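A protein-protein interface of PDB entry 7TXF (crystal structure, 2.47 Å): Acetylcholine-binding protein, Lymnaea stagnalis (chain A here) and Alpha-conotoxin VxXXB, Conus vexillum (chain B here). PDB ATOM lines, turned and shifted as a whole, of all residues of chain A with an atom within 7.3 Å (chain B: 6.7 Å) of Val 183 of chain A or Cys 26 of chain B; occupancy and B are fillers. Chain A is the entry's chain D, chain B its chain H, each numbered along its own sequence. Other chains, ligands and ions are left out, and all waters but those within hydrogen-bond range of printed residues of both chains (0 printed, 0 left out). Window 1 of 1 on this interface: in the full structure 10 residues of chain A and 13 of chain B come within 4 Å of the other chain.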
ATOM      1  N   TYR A  89      -7.377 -29.023  31.994  1.00  0.00           N
ATOM      2  CA  TYR A  89      -8.617 -28.801  31.198  1.00  0.00           C
ATOM      3  C   TYR A  89      -9.633 -29.933  31.432  1.00  0.00           C
ATOM      4  O   TYR A  89     -10.832 -29.667  31.335  1.00  0.00           O
ATOM      5  CB  TYR A  89      -8.302 -28.653  29.702  1.00  0.00           C
ATOM      6  CG  TYR A  89      -7.444 -27.477  29.310  1.00  0.00           C
ATOM      7  CD1 TYR A  89      -7.104 -26.485  30.213  1.00  0.00           C
ATOM      8  CD2 TYR A  89      -6.981 -27.339  28.016  1.00  0.00           C
ATOM      9  CE1 TYR A  89      -6.318 -25.408  29.848  1.00  0.00           C
ATOM     10  CE2 TYR A  89      -6.182 -26.272  27.635  1.00  0.00           C
ATOM     11  CZ  TYR A  89      -5.844 -25.300  28.557  1.00  0.00           C
ATOM     12  OH  TYR A  89      -5.077 -24.227  28.208  1.00  0.00           O
ATOM     13  N   LYS A 139      -4.217 -32.600  30.292  1.00  0.00           N
ATOM     14  CA  LYS A 139      -3.926 -31.413  29.502  1.00  0.00           C
ATOM     15  C   LYS A 139      -3.819 -30.226  30.441  1.00  0.00           C
ATOM     16  O   LYS A 139      -4.779 -29.914  31.104  1.00  0.00           O
ATOM     17  CB  LYS A 139      -5.036 -31.201  28.479  1.00  0.00           C
ATOM     18  CG  LYS A 139      -4.520 -30.577  27.206  1.00  0.00           C
ATOM     19  CD  LYS A 139      -5.659 -30.243  26.235  1.00  0.00           C
ATOM     20  CE  LYS A 139      -6.111 -31.389  25.330  1.00  0.00           C
ATOM     21  NZ  LYS A 139      -4.971 -32.138  24.767  1.00  0.00           N
ATOM     22  N   HIS A 146      -3.474 -16.204  26.843  1.00  0.00           N
ATOM     23  CA  HIS A 146      -2.978 -16.747  25.584  1.00  0.00           C
ATOM     24  C   HIS A 146      -1.467 -16.565  25.431  1.00  0.00           C
ATOM     25  O   HIS A 146      -0.798 -16.034  26.270  1.00  0.00           O
ATOM     26  CB  HIS A 146      -3.719 -16.115  24.395  1.00  0.00           C
ATOM     27  CG  HIS A 146      -3.690 -14.620  24.390  1.00  0.00           C
ATOM     28  ND1 HIS A 146      -2.518 -13.896  24.396  1.00  0.00           N
ATOM     29  CD2 HIS A 146      -4.689 -13.715  24.311  1.00  0.00           C
ATOM     30  CE1 HIS A 146      -2.793 -12.612  24.351  1.00  0.00           C
ATOM     31  NE2 HIS A 146      -4.105 -12.474  24.327  1.00  0.00           N
ATOM     32  N   SER A 147      -0.948 -17.001  24.282  1.00  0.00           N
ATOM     33  CA  SER A 147       0.478 -17.190  24.017  1.00  0.00           C
ATOM     34  C   SER A 147       1.307 -15.921  23.976  1.00  0.00           C
ATOM     35  O   SER A 147       2.518 -16.001  24.166  1.00  0.00           O
ATOM     36  CB  SER A 147       0.678 -17.996  22.735  1.00  0.00           C
ATOM     37  OG  SER A 147       0.088 -17.306  21.663  1.00  0.00           O
ATOM     38  N   ASN A 181       1.066 -28.465  22.838  1.00  0.00           N
ATOM     39  CA  ASN A 181       0.108 -28.005  21.842  1.00  0.00           C
ATOM     40  C   ASN A 181      -0.092 -26.504  21.870  1.00  0.00           C
ATOM     41  O   ASN A 181       0.062 -25.867  22.888  1.00  0.00           O
ATOM     42  CB  ASN A 181      -1.263 -28.591  22.078  1.00  0.00           C
ATOM     43  CG  ASN A 181      -1.280 -30.058  21.927  1.00  0.00           C
ATOM     44  OD1 ASN A 181      -1.066 -30.578  20.827  1.00  0.00           O
ATOM     45  ND2 ASN A 181      -1.539 -30.750  23.032  1.00  0.00           N
ATOM     46  N   SER A 182      -0.471 -25.995  20.697  1.00  0.00           N
ATOM     47  CA  SER A 182      -0.855 -24.648  20.423  1.00  0.00           C
ATOM     48  C   SER A 182      -2.204 -24.748  19.739  1.00  0.00           C
ATOM     49  O   SER A 182      -2.317 -25.304  18.638  1.00  0.00           O
ATOM     50  CB  SER A 182       0.136 -24.034  19.439  1.00  0.00           C
ATOM     51  OG  SER A 182       1.383 -23.755  20.062  1.00  0.00           O
ATOM     52  N   VAL A 183      -3.228 -24.218  20.408  1.00  0.00           N
ATOM     53  CA  VAL A 183      -4.583 -24.147  19.885  1.00  0.00           C
ATOM     54  C   VAL A 183      -4.822 -22.719  19.346  1.00  0.00           C
ATOM     55  O   VAL A 183      -4.591 -21.737  20.079  1.00  0.00           O
ATOM     56  CB  VAL A 183      -5.596 -24.487  21.010  1.00  0.00           C
ATOM     57  CG1 VAL A 183      -6.992 -24.637  20.406  1.00  0.00           C
ATOM     58  CG2 VAL A 183      -5.161 -25.715  21.790  1.00  0.00           C
ATOM     59  N   THR A 184      -5.286 -22.606  18.096  1.00  0.00           N
ATOM     60  CA  THR A 184      -5.622 -21.303  17.524  1.00  0.00           C
ATOM     61  C   THR A 184      -7.063 -21.270  17.028  1.00  0.00           C
ATOM     62  O   THR A 184      -7.538 -22.249  16.502  1.00  0.00           O
ATOM     63  CB  THR A 184      -4.645 -20.834  16.430  1.00  0.00           C
ATOM     64  OG1 THR A 184      -4.610 -21.773  15.361  1.00  0.00           O
ATOM     65  CG2 THR A 184      -3.251 -20.661  17.018  1.00  0.00           C
ATOM     66  N   TYR A 185      -7.718 -20.136  17.274  1.00  0.00           N
ATOM     67  CA  TYR A 185      -9.173 -19.914  17.082  1.00  0.00           C
ATOM     68  C   TYR A 185      -9.371 -18.750  16.096  1.00  0.00           C
ATOM     69  O   TYR A 185      -8.495 -17.893  16.010  1.00  0.00           O
ATOM     70  CB  TYR A 185      -9.857 -19.625  18.413  1.00  0.00           C
ATOM     71  CG  TYR A 185      -9.660 -20.650  19.496  1.00  0.00           C
ATOM     72  CD1 TYR A 185     -10.564 -21.687  19.676  1.00  0.00           C
ATOM     73  CD2 TYR A 185      -8.644 -20.508  20.424  1.00  0.00           C
ATOM     74  CE1 TYR A 185     -10.416 -22.602  20.707  1.00  0.00           C
ATOM     75  CE2 TYR A 185      -8.495 -21.400  21.480  1.00  0.00           C
ATOM     76  CZ  TYR A 185      -9.396 -22.439  21.631  1.00  0.00           C
ATOM     77  OH  TYR A 185      -9.248 -23.316  22.669  1.00  0.00           O
ATOM     78  N   SER A 186     -10.483 -18.784  15.356  1.00  0.00           N
ATOM     79  CA  SER A 186     -10.746 -17.899  14.242  1.00  0.00           C
ATOM     80  C   SER A 186     -10.919 -16.436  14.614  1.00  0.00           C
ATOM     81  O   SER A 186     -10.784 -15.588  13.738  1.00  0.00           O
ATOM     82  CB  SER A 186     -11.970 -18.396  13.438  1.00  0.00           C
ATOM     83  OG  SER A 186     -12.865 -19.199  14.219  1.00  0.00           O
ATOM     84  N   CYS A 188      -9.016 -14.671  16.789  1.00  0.00           N
ATOM     85  CA  CYS A 188      -7.873 -14.031  17.413  1.00  0.00           C
ATOM     86  C   CYS A 188      -6.570 -14.533  16.810  1.00  0.00           C
ATOM     87  O   CYS A 188      -6.453 -15.706  16.477  1.00  0.00           O
ATOM     88  CB  CYS A 188      -7.952 -14.367  18.903  1.00  0.00           C
ATOM     89  SG  CYS A 188      -9.520 -13.944  19.668  1.00  0.00           S
ATOM     90  N   GLU A 190      -3.755 -14.786  18.433  1.00  0.00           N
ATOM     91  CA  GLU A 190      -2.981 -15.385  19.496  1.00  0.00           C
ATOM     92  C   GLU A 190      -3.449 -16.819  19.751  1.00  0.00           C
ATOM     93  O   GLU A 190      -4.573 -17.192  19.421  1.00  0.00           O
ATOM     94  CB  GLU A 190      -3.029 -14.571  20.795  1.00  0.00           C
ATOM     95  CG  GLU A 190      -2.752 -13.068  20.700  1.00  0.00           C
ATOM     96  CD  GLU A 190      -3.989 -12.228  20.383  1.00  0.00           C
ATOM     97  OE1 GLU A 190      -5.103 -12.784  20.209  1.00  0.00           O
ATOM     98  OE2 GLU A 190      -3.845 -10.970  20.330  1.00  0.00           O
ATOM     99  N   ALA A 191      -2.545 -17.612  20.336  1.00  0.00           N
ATOM    100  CA  ALA A 191      -2.710 -19.051  20.530  1.00  0.00           C
ATOM    101  C   ALA A 191      -2.834 -19.403  22.018  1.00  0.00           C
ATOM    102  O   ALA A 191      -2.363 -18.673  22.851  1.00  0.00           O
ATOM    103  CB  ALA A 191      -1.507 -19.756  19.908  1.00  0.00           C
ATOM    104  N   TYR A 192      -3.436 -20.548  22.326  1.00  0.00           N
ATOM    105  CA  TYR A 192      -3.536 -21.081  23.710  1.00  0.00           C
ATOM    106  C   TYR A 192      -2.698 -22.341  23.834  1.00  0.00           C
ATOM    107  O   TYR A 192      -2.946 -23.283  23.078  1.00  0.00           O
ATOM    108  CB  TYR A 192      -5.003 -21.274  24.070  1.00  0.00           C
ATOM    109  CG  TYR A 192      -5.721 -19.953  24.103  1.00  0.00           C
ATOM    110  CD1 TYR A 192      -6.102 -19.334  22.915  1.00  0.00           C
ATOM    111  CD2 TYR A 192      -5.928 -19.286  25.304  1.00  0.00           C
ATOM    112  CE1 TYR A 192      -6.744 -18.109  22.931  1.00  0.00           C
ATOM    113  CE2 TYR A 192      -6.551 -18.048  25.332  1.00  0.00           C
ATOM    114  CZ  TYR A 192      -6.973 -17.470  24.146  1.00  0.00           C
ATOM    115  OH  TYR A 192      -7.596 -16.263  24.189  1.00  0.00           O
ATOM    116  N   GLU A 193      -1.696 -22.303  24.709  1.00  0.00           N
ATOM    117  CA  GLU A 193      -0.688 -23.331  24.787  1.00  0.00           C
ATOM    118  C   GLU A 193      -0.975 -24.237  25.986  1.00  0.00           C
ATOM    119  O   GLU A 193      -1.389 -23.755  27.068  1.00  0.00           O
ATOM    120  CB  GLU A 193       0.713 -22.694  24.851  1.00  0.00           C
ATOM    121  CG  GLU A 193       1.055 -21.940  23.544  1.00  0.00           C
ATOM    122  CD  GLU A 193       2.498 -21.454  23.441  1.00  0.00           C
ATOM    123  OE1 GLU A 193       3.225 -21.540  24.430  1.00  0.00           O
ATOM    124  OE2 GLU A 193       2.994 -21.089  22.368  1.00  0.00           O
ATOM    125  N   ASP A 194      -0.775 -25.542  25.782  1.00  0.00           N
ATOM    126  CA  ASP A 194      -0.868 -26.520  26.859  1.00  0.00           C
ATOM    127  C   ASP A 194       0.213 -27.565  26.727  1.00  0.00           C
ATOM    128  O   ASP A 194       0.832 -27.709  25.662  1.00  0.00           O
ATOM    129  CB  ASP A 194      -2.235 -27.228  26.855  1.00  0.00           C
ATOM    130  CG  ASP A 194      -2.504 -27.973  25.561  1.00  0.00           C
ATOM    131  OD1 ASP A 194      -1.988 -29.088  25.326  1.00  0.00           O
ATOM    132  OD2 ASP A 194      -3.238 -27.396  24.748  1.00  0.00           O
ATOM    133  N   ARG B   2      -6.737 -30.880   8.524  1.00  0.00           N
ATOM    134  CA  ARG B   2      -8.084 -30.701   9.112  1.00  0.00           C
ATOM    135  C   ARG B   2      -8.622 -29.309   8.734  1.00  0.00           C
ATOM    136  O   ARG B   2      -7.873 -28.303   8.806  1.00  0.00           O
ATOM    137  CB  ARG B   2      -8.054 -30.868  10.639  1.00  0.00           C
ATOM    138  CG  ARG B   2      -7.279 -32.064  11.165  1.00  0.00           C
ATOM    139  CD  ARG B   2      -7.781 -33.420  10.701  1.00  0.00           C
ATOM    140  NE  ARG B   2      -7.352 -34.444  11.645  1.00  0.00           N
ATOM    141  CZ  ARG B   2      -6.131 -34.996  11.700  1.00  0.00           C
ATOM    142  NH1 ARG B   2      -5.178 -34.628  10.855  1.00  0.00           N
ATOM    143  NH2 ARG B   2      -5.867 -35.911  12.618  1.00  0.00           N
ATOM    144  N   MET B   3      -9.918 -29.263   8.413  1.00  0.00           N
ATOM    145  CA  MET B   3     -10.732 -28.072   8.541  1.00  0.00           C
ATOM    146  C   MET B   3     -11.619 -28.256   9.777  1.00  0.00           C
ATOM    147  O   MET B   3     -12.305 -29.283   9.929  1.00  0.00           O
ATOM    148  CB  MET B   3     -11.567 -27.900   7.285  1.00  0.00           C
ATOM    149  CG  MET B   3     -12.518 -26.716   7.243  1.00  0.00           C
ATOM    150  SD  MET B   3     -12.052 -25.137   6.472  1.00  0.00           S
ATOM    151  CE  MET B   3     -10.731 -25.574   5.332  1.00  0.00           C
ATOM    152  N   CYS B   4     -11.548 -27.273  10.681  1.00  0.00           N
ATOM    153  CA  CYS B   4     -12.329 -27.218  11.912  1.00  0.00           C
ATOM    154  C   CYS B   4     -13.205 -25.982  11.811  1.00  0.00           C
ATOM    155  O   CYS B   4     -12.698 -24.878  11.964  1.00  0.00           O
ATOM    156  CB  CYS B   4     -11.383 -27.099  13.110  1.00  0.00           C
ATOM    157  SG  CYS B   4     -10.239 -28.496  13.316  1.00  0.00           S
ATOM    158  N   MET B   7     -11.987 -22.720  10.210  1.00  0.00           N
ATOM    159  CA  MET B   7     -10.534 -22.760  10.326  1.00  0.00           C
ATOM    160  C   MET B   7      -9.851 -23.902   9.548  1.00  0.00           C
ATOM    161  O   MET B   7     -10.204 -25.076   9.676  1.00  0.00           O
ATOM    162  CB  MET B   7     -10.109 -22.836  11.791  1.00  0.00           C
ATOM    163  CG  MET B   7      -8.600 -22.713  11.984  1.00  0.00           C
ATOM    164  SD  MET B   7      -7.911 -21.759  13.364  1.00  0.00           S
ATOM    165  CE  MET B   7      -6.226 -21.440  12.788  1.00  0.00           C
ATOM    166  N   SER B   8      -8.841 -23.522   8.758  1.00  0.00           N
ATOM    167  CA  SER B   8      -7.920 -24.450   8.120  1.00  0.00           C
ATOM    168  C   SER B   8      -6.711 -24.589   9.069  1.00  0.00           C
ATOM    169  O   SER B   8      -6.141 -23.582   9.494  1.00  0.00           O
ATOM    170  CB  SER B   8      -7.500 -23.889   6.763  1.00  0.00           C
ATOM    171  OG  SER B   8      -7.092 -24.927   5.917  1.00  0.00           O
ATOM    172  N   CYS B   9      -6.339 -25.824   9.419  1.00  0.00           N
ATOM    173  CA  CYS B   9      -5.301 -26.052  10.431  1.00  0.00           C
ATOM    174  C   CYS B   9      -3.887 -25.798   9.917  1.00  0.00           C
ATOM    175  O   CYS B   9      -3.562 -26.201   8.805  1.00  0.00           O
ATOM    176  CB  CYS B   9      -5.402 -27.452  11.000  1.00  0.00           C
ATOM    177  SG  CYS B   9      -6.912 -27.773  11.960  1.00  0.00           S
ATOM    178  N   PRO B  10      -3.012 -25.135  10.719  1.00  0.00           N
ATOM    179  CA  PRO B  10      -1.675 -24.742  10.270  1.00  0.00           C
ATOM    180  C   PRO B  10      -0.715 -25.881   9.888  1.00  0.00           C
ATOM    181  O   PRO B  10       0.163 -25.611   9.095  1.00  0.00           O
ATOM    182  CB  PRO B  10      -1.079 -23.993  11.477  1.00  0.00           C
ATOM    183  CG  PRO B  10      -2.275 -23.545  12.279  1.00  0.00           C
ATOM    184  CD  PRO B  10      -3.282 -24.661  12.085  1.00  0.00           C
ATOM    185  N   CYS B  14      -3.399 -32.159  13.767  1.00  0.00           N
ATOM    186  CA  CYS B  14      -4.187 -31.227  14.528  1.00  0.00           C
ATOM    187  C   CYS B  14      -5.567 -31.836  14.728  1.00  0.00           C
ATOM    188  O   CYS B  14      -6.074 -32.522  13.844  1.00  0.00           O
ATOM    189  CB  CYS B  14      -4.294 -29.852  13.816  1.00  0.00           C
ATOM    190  SG  CYS B  14      -2.730 -28.937  13.522  1.00  0.00           S
ATOM    191  N   THR B  15      -6.173 -31.541  15.883  1.00  0.00           N
ATOM    192  CA  THR B  15      -7.552 -31.898  16.218  1.00  0.00           C
ATOM    193  C   THR B  15      -8.438 -30.605  16.286  1.00  0.00           C
ATOM    194  O   THR B  15      -7.899 -29.493  16.336  1.00  0.00           O
ATOM    195  CB  THR B  15      -7.602 -32.764  17.534  1.00  0.00           C
ATOM    196  OG1 THR B  15      -7.674 -31.945  18.713  1.00  0.00           O
ATOM    197  CG2 THR B  15      -6.393 -33.687  17.670  1.00  0.00           C
ATOM    198  N   CYS B  16      -9.766 -30.764  16.279  1.00  0.00           N
ATOM    199  CA  CYS B  16     -10.696 -29.642  16.302  1.00  0.00           C
ATOM    200  C   CYS B  16     -11.175 -29.313  17.707  1.00  0.00           C
ATOM    201  O   CYS B  16     -11.285 -30.207  18.536  1.00  0.00           O
ATOM    202  CB  CYS B  16     -11.898 -29.953  15.413  1.00  0.00           C
ATOM    203  SG  CYS B  16     -11.527 -30.036  13.641  1.00  0.00           S
ATOM    204  N   VAL B  17     -11.442 -28.021  17.949  1.00  0.00           N
ATOM    205  CA  VAL B  17     -12.042 -27.484  19.182  1.00  0.00           C
ATOM    206  C   VAL B  17     -12.951 -26.295  18.851  1.00  0.00           C
ATOM    207  O   VAL B  17     -12.780 -25.649  17.820  1.00  0.00           O
ATOM    208  CB  VAL B  17     -10.954 -27.000  20.180  1.00  0.00           C
ATOM    209  CG1 VAL B  17     -10.051 -28.168  20.588  1.00  0.00           C
ATOM    210  CG2 VAL B  17     -10.141 -25.825  19.600  1.00  0.00           C
ATOM    211  N   HIS B  24     -14.302 -21.577  16.257  1.00  0.00           N
ATOM    212  CA  HIS B  24     -13.671 -22.838  15.858  1.00  0.00           C
ATOM    213  C   HIS B  24     -12.155 -22.702  15.903  1.00  0.00           C
ATOM    214  O   HIS B  24     -11.618 -21.650  15.556  1.00  0.00           O
ATOM    215  CB  HIS B  24     -14.110 -23.231  14.445  1.00  0.00           C
ATOM    216  CG  HIS B  24     -15.562 -23.574  14.340  1.00  0.00           C
ATOM    217  ND1 HIS B  24     -16.078 -24.791  14.748  1.00  0.00           N
ATOM    218  CD2 HIS B  24     -16.609 -22.851  13.883  1.00  0.00           C
ATOM    219  CE1 HIS B  24     -17.384 -24.800  14.543  1.00  0.00           C
ATOM    220  NE2 HIS B  24     -17.729 -23.637  14.016  1.00  0.00           N
ATOM    221  N   GLY B  25     -11.480 -23.770  16.330  1.00  0.00           N
ATOM    222  CA  GLY B  25     -10.040 -23.771  16.469  1.00  0.00           C
ATOM    223  C   GLY B  25      -9.385 -25.082  16.115  1.00  0.00           C
ATOM    224  O   GLY B  25     -10.045 -26.120  16.012  1.00  0.00           O
ATOM    225  N   CYS B  26      -8.061 -25.017  15.921  1.00  0.00           N
ATOM    226  CA  CYS B  26      -7.209 -26.177  15.714  1.00  0.00           C
ATOM    227  C   CYS B  26      -6.245 -26.332  16.864  1.00  0.00           C
ATOM    228  O   CYS B  26      -5.480 -25.419  17.152  1.00  0.00           O
ATOM    229  CB  CYS B  26      -6.413 -25.997  14.428  1.00  0.00           C
ATOM    230  SG  CYS B  26      -7.446 -26.027  12.936  1.00  0.00           S
ATOM    231  N   SER B  27      -6.291 -27.493  17.525  1.00  0.00           N
ATOM    232  CA  SER B  27      -5.304 -27.864  18.534  1.00  0.00           C
ATOM    233  C   SER B  27      -4.200 -28.626  17.822  1.00  0.00           C
ATOM    234  O   SER B  27      -4.433 -29.716  17.360  1.00  0.00           O
ATOM    235  CB  SER B  27      -5.906 -28.729  19.636  1.00  0.00           C
ATOM    236  OG  SER B  27      -4.884 -29.042  20.565  1.00  0.00           O
ATOM    237  N   CYS B  28      -3.009 -28.020  17.752  1.00  0.00           N
ATOM    238  CA  CYS B  28      -1.911 -28.521  16.968  1.00  0.00           C
ATOM    239  C   CYS B  28      -0.703 -28.973  17.779  1.00  0.00           C
ATOM    240  O   CYS B  28      -0.368 -28.372  18.788  1.00  0.00           O
ATOM    241  CB  CYS B  28      -1.516 -27.444  15.967  1.00  0.00           C
ATOM    242  SG  CYS B  28      -2.831 -27.235  14.737  1.00  0.00           S
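The backbone carbonyl oxygen (O) of Ser 182 of chain A sits close to the backbone carbonyl oxygen (O) of Cys 26 of chain B.
The backbone carbonyl oxygen (O) of Thr 184 of chain A sits close to the side-chain sulfur (SD) of Met 7 of chain B, 3.2 Å away.
The backbone carbonyl oxygen (O) of His 24 of chain B lies within hydrogen-bond range of the side-chain hydroxyl (OG) of Ser 186 of chain A (3.1 Å).
The backbone carbonyl oxygen of Thr 184 of chain A is in hydrogen-bond range of the backbone NH of Cys 26 of chain B, 2.9 Å away.
The backbone NH (N) of Cys 28 of chain B is in hydrogen-bond range of the backbone carbonyl oxygen (O) of Ser 182 of chain A (2.9 Å).
OD1 of Asn 181 of chain A lies close to O of Cys 28 of chain B (3.1 Å).
Ser 27 of chain B touches Asn 181 of chain A.
O of Ser 182 of chain A touches C of Ser 27 of chain B, at 3.9 Å.
Val 17 of chain B touches Val 183 of chain A.
Val 183 of chain A touches Cys 26 of chain B (CA to O, 3.1 Å).
Ser 27 of chain B touches Val 183 of chain A (OG to CG2, 3.6 Å).
O of Thr 184 of chain A touches CA of Gly 25 of chain B, 2.9 Å away.
Tyr 185 of chain A touches Val 17 of chain B (CE1 to CG2, 3.4 Å).
His 24 of chain B touches Tyr 185 of chain A.
Gly 25 of chain B touches Tyr 185 of chain A.
Of the 16 printed residues of chain B, 7 touch a printed residue of chain A.
Printed residues of chain B that touch a printed residue of chain A: Met 7, Val 17, His 24, Gly 25, Cys 26, Ser 27 and Cys 28.
Hydrophobic or aromatic side chains of chain B within 4 Å of the printed part of chain A: Met 7 and Val 17.
Of the 16 printed residues of chain A, 6 touch a printed residue of chain B.
Along chain A the printed residues that touch a printed residue of chain B span positions 181 to 186.
Among the printed residues, 15 pairs touch across the chains.
Among the printed residues, no Asp or Glu carboxylate lies within 4 Å of a Lys or Arg side-chain nitrogen of the other chain.
Val 183 of chain A touches three residues of chain B.
Of the printed residues of chain B, Ser 186 of chain A touches His 24 (3.1 Å).
Printed residues of chain A within 4 Å of Met 7 of chain B: Thr 184 (3.1 Å).
Of chain A, only Ser 182 (3.5 Å), Val 183 (3.1 Å) and Thr 184 (2.9 Å) come within 4 Å of Cys 26 of chain B.
The nearest printed residue of chain A that does not touch Met 7 of chain B is Tyr 185 of chain A (4.2 Å).
SG of Cys 26 of chain B forms a disulfide with SG of Cys 9 of chain B (2.1 Å).
N of Ser 27 of chain B is in hydrogen-bond range of O of Thr 15 of chain B (2.8 Å).
SG of Cys 4 of chain B is disulfide-bonded to SG of Cys 16 of chain B, at 2.0 Å.
The side-chain amide nitrogen (ND2) of Asn 181 of chain A lies within hydrogen-bond range of the side-chain carboxylate (OD1) of Asp 194 of chain A, 2.9 Å away.
O of Val 183 of chain A lies within hydrogen-bond range of N of Tyr 192 of chain A (2.8 Å).
SG of Cys 14 of chain B forms a disulfide with SG of Cys 28 of chain B.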
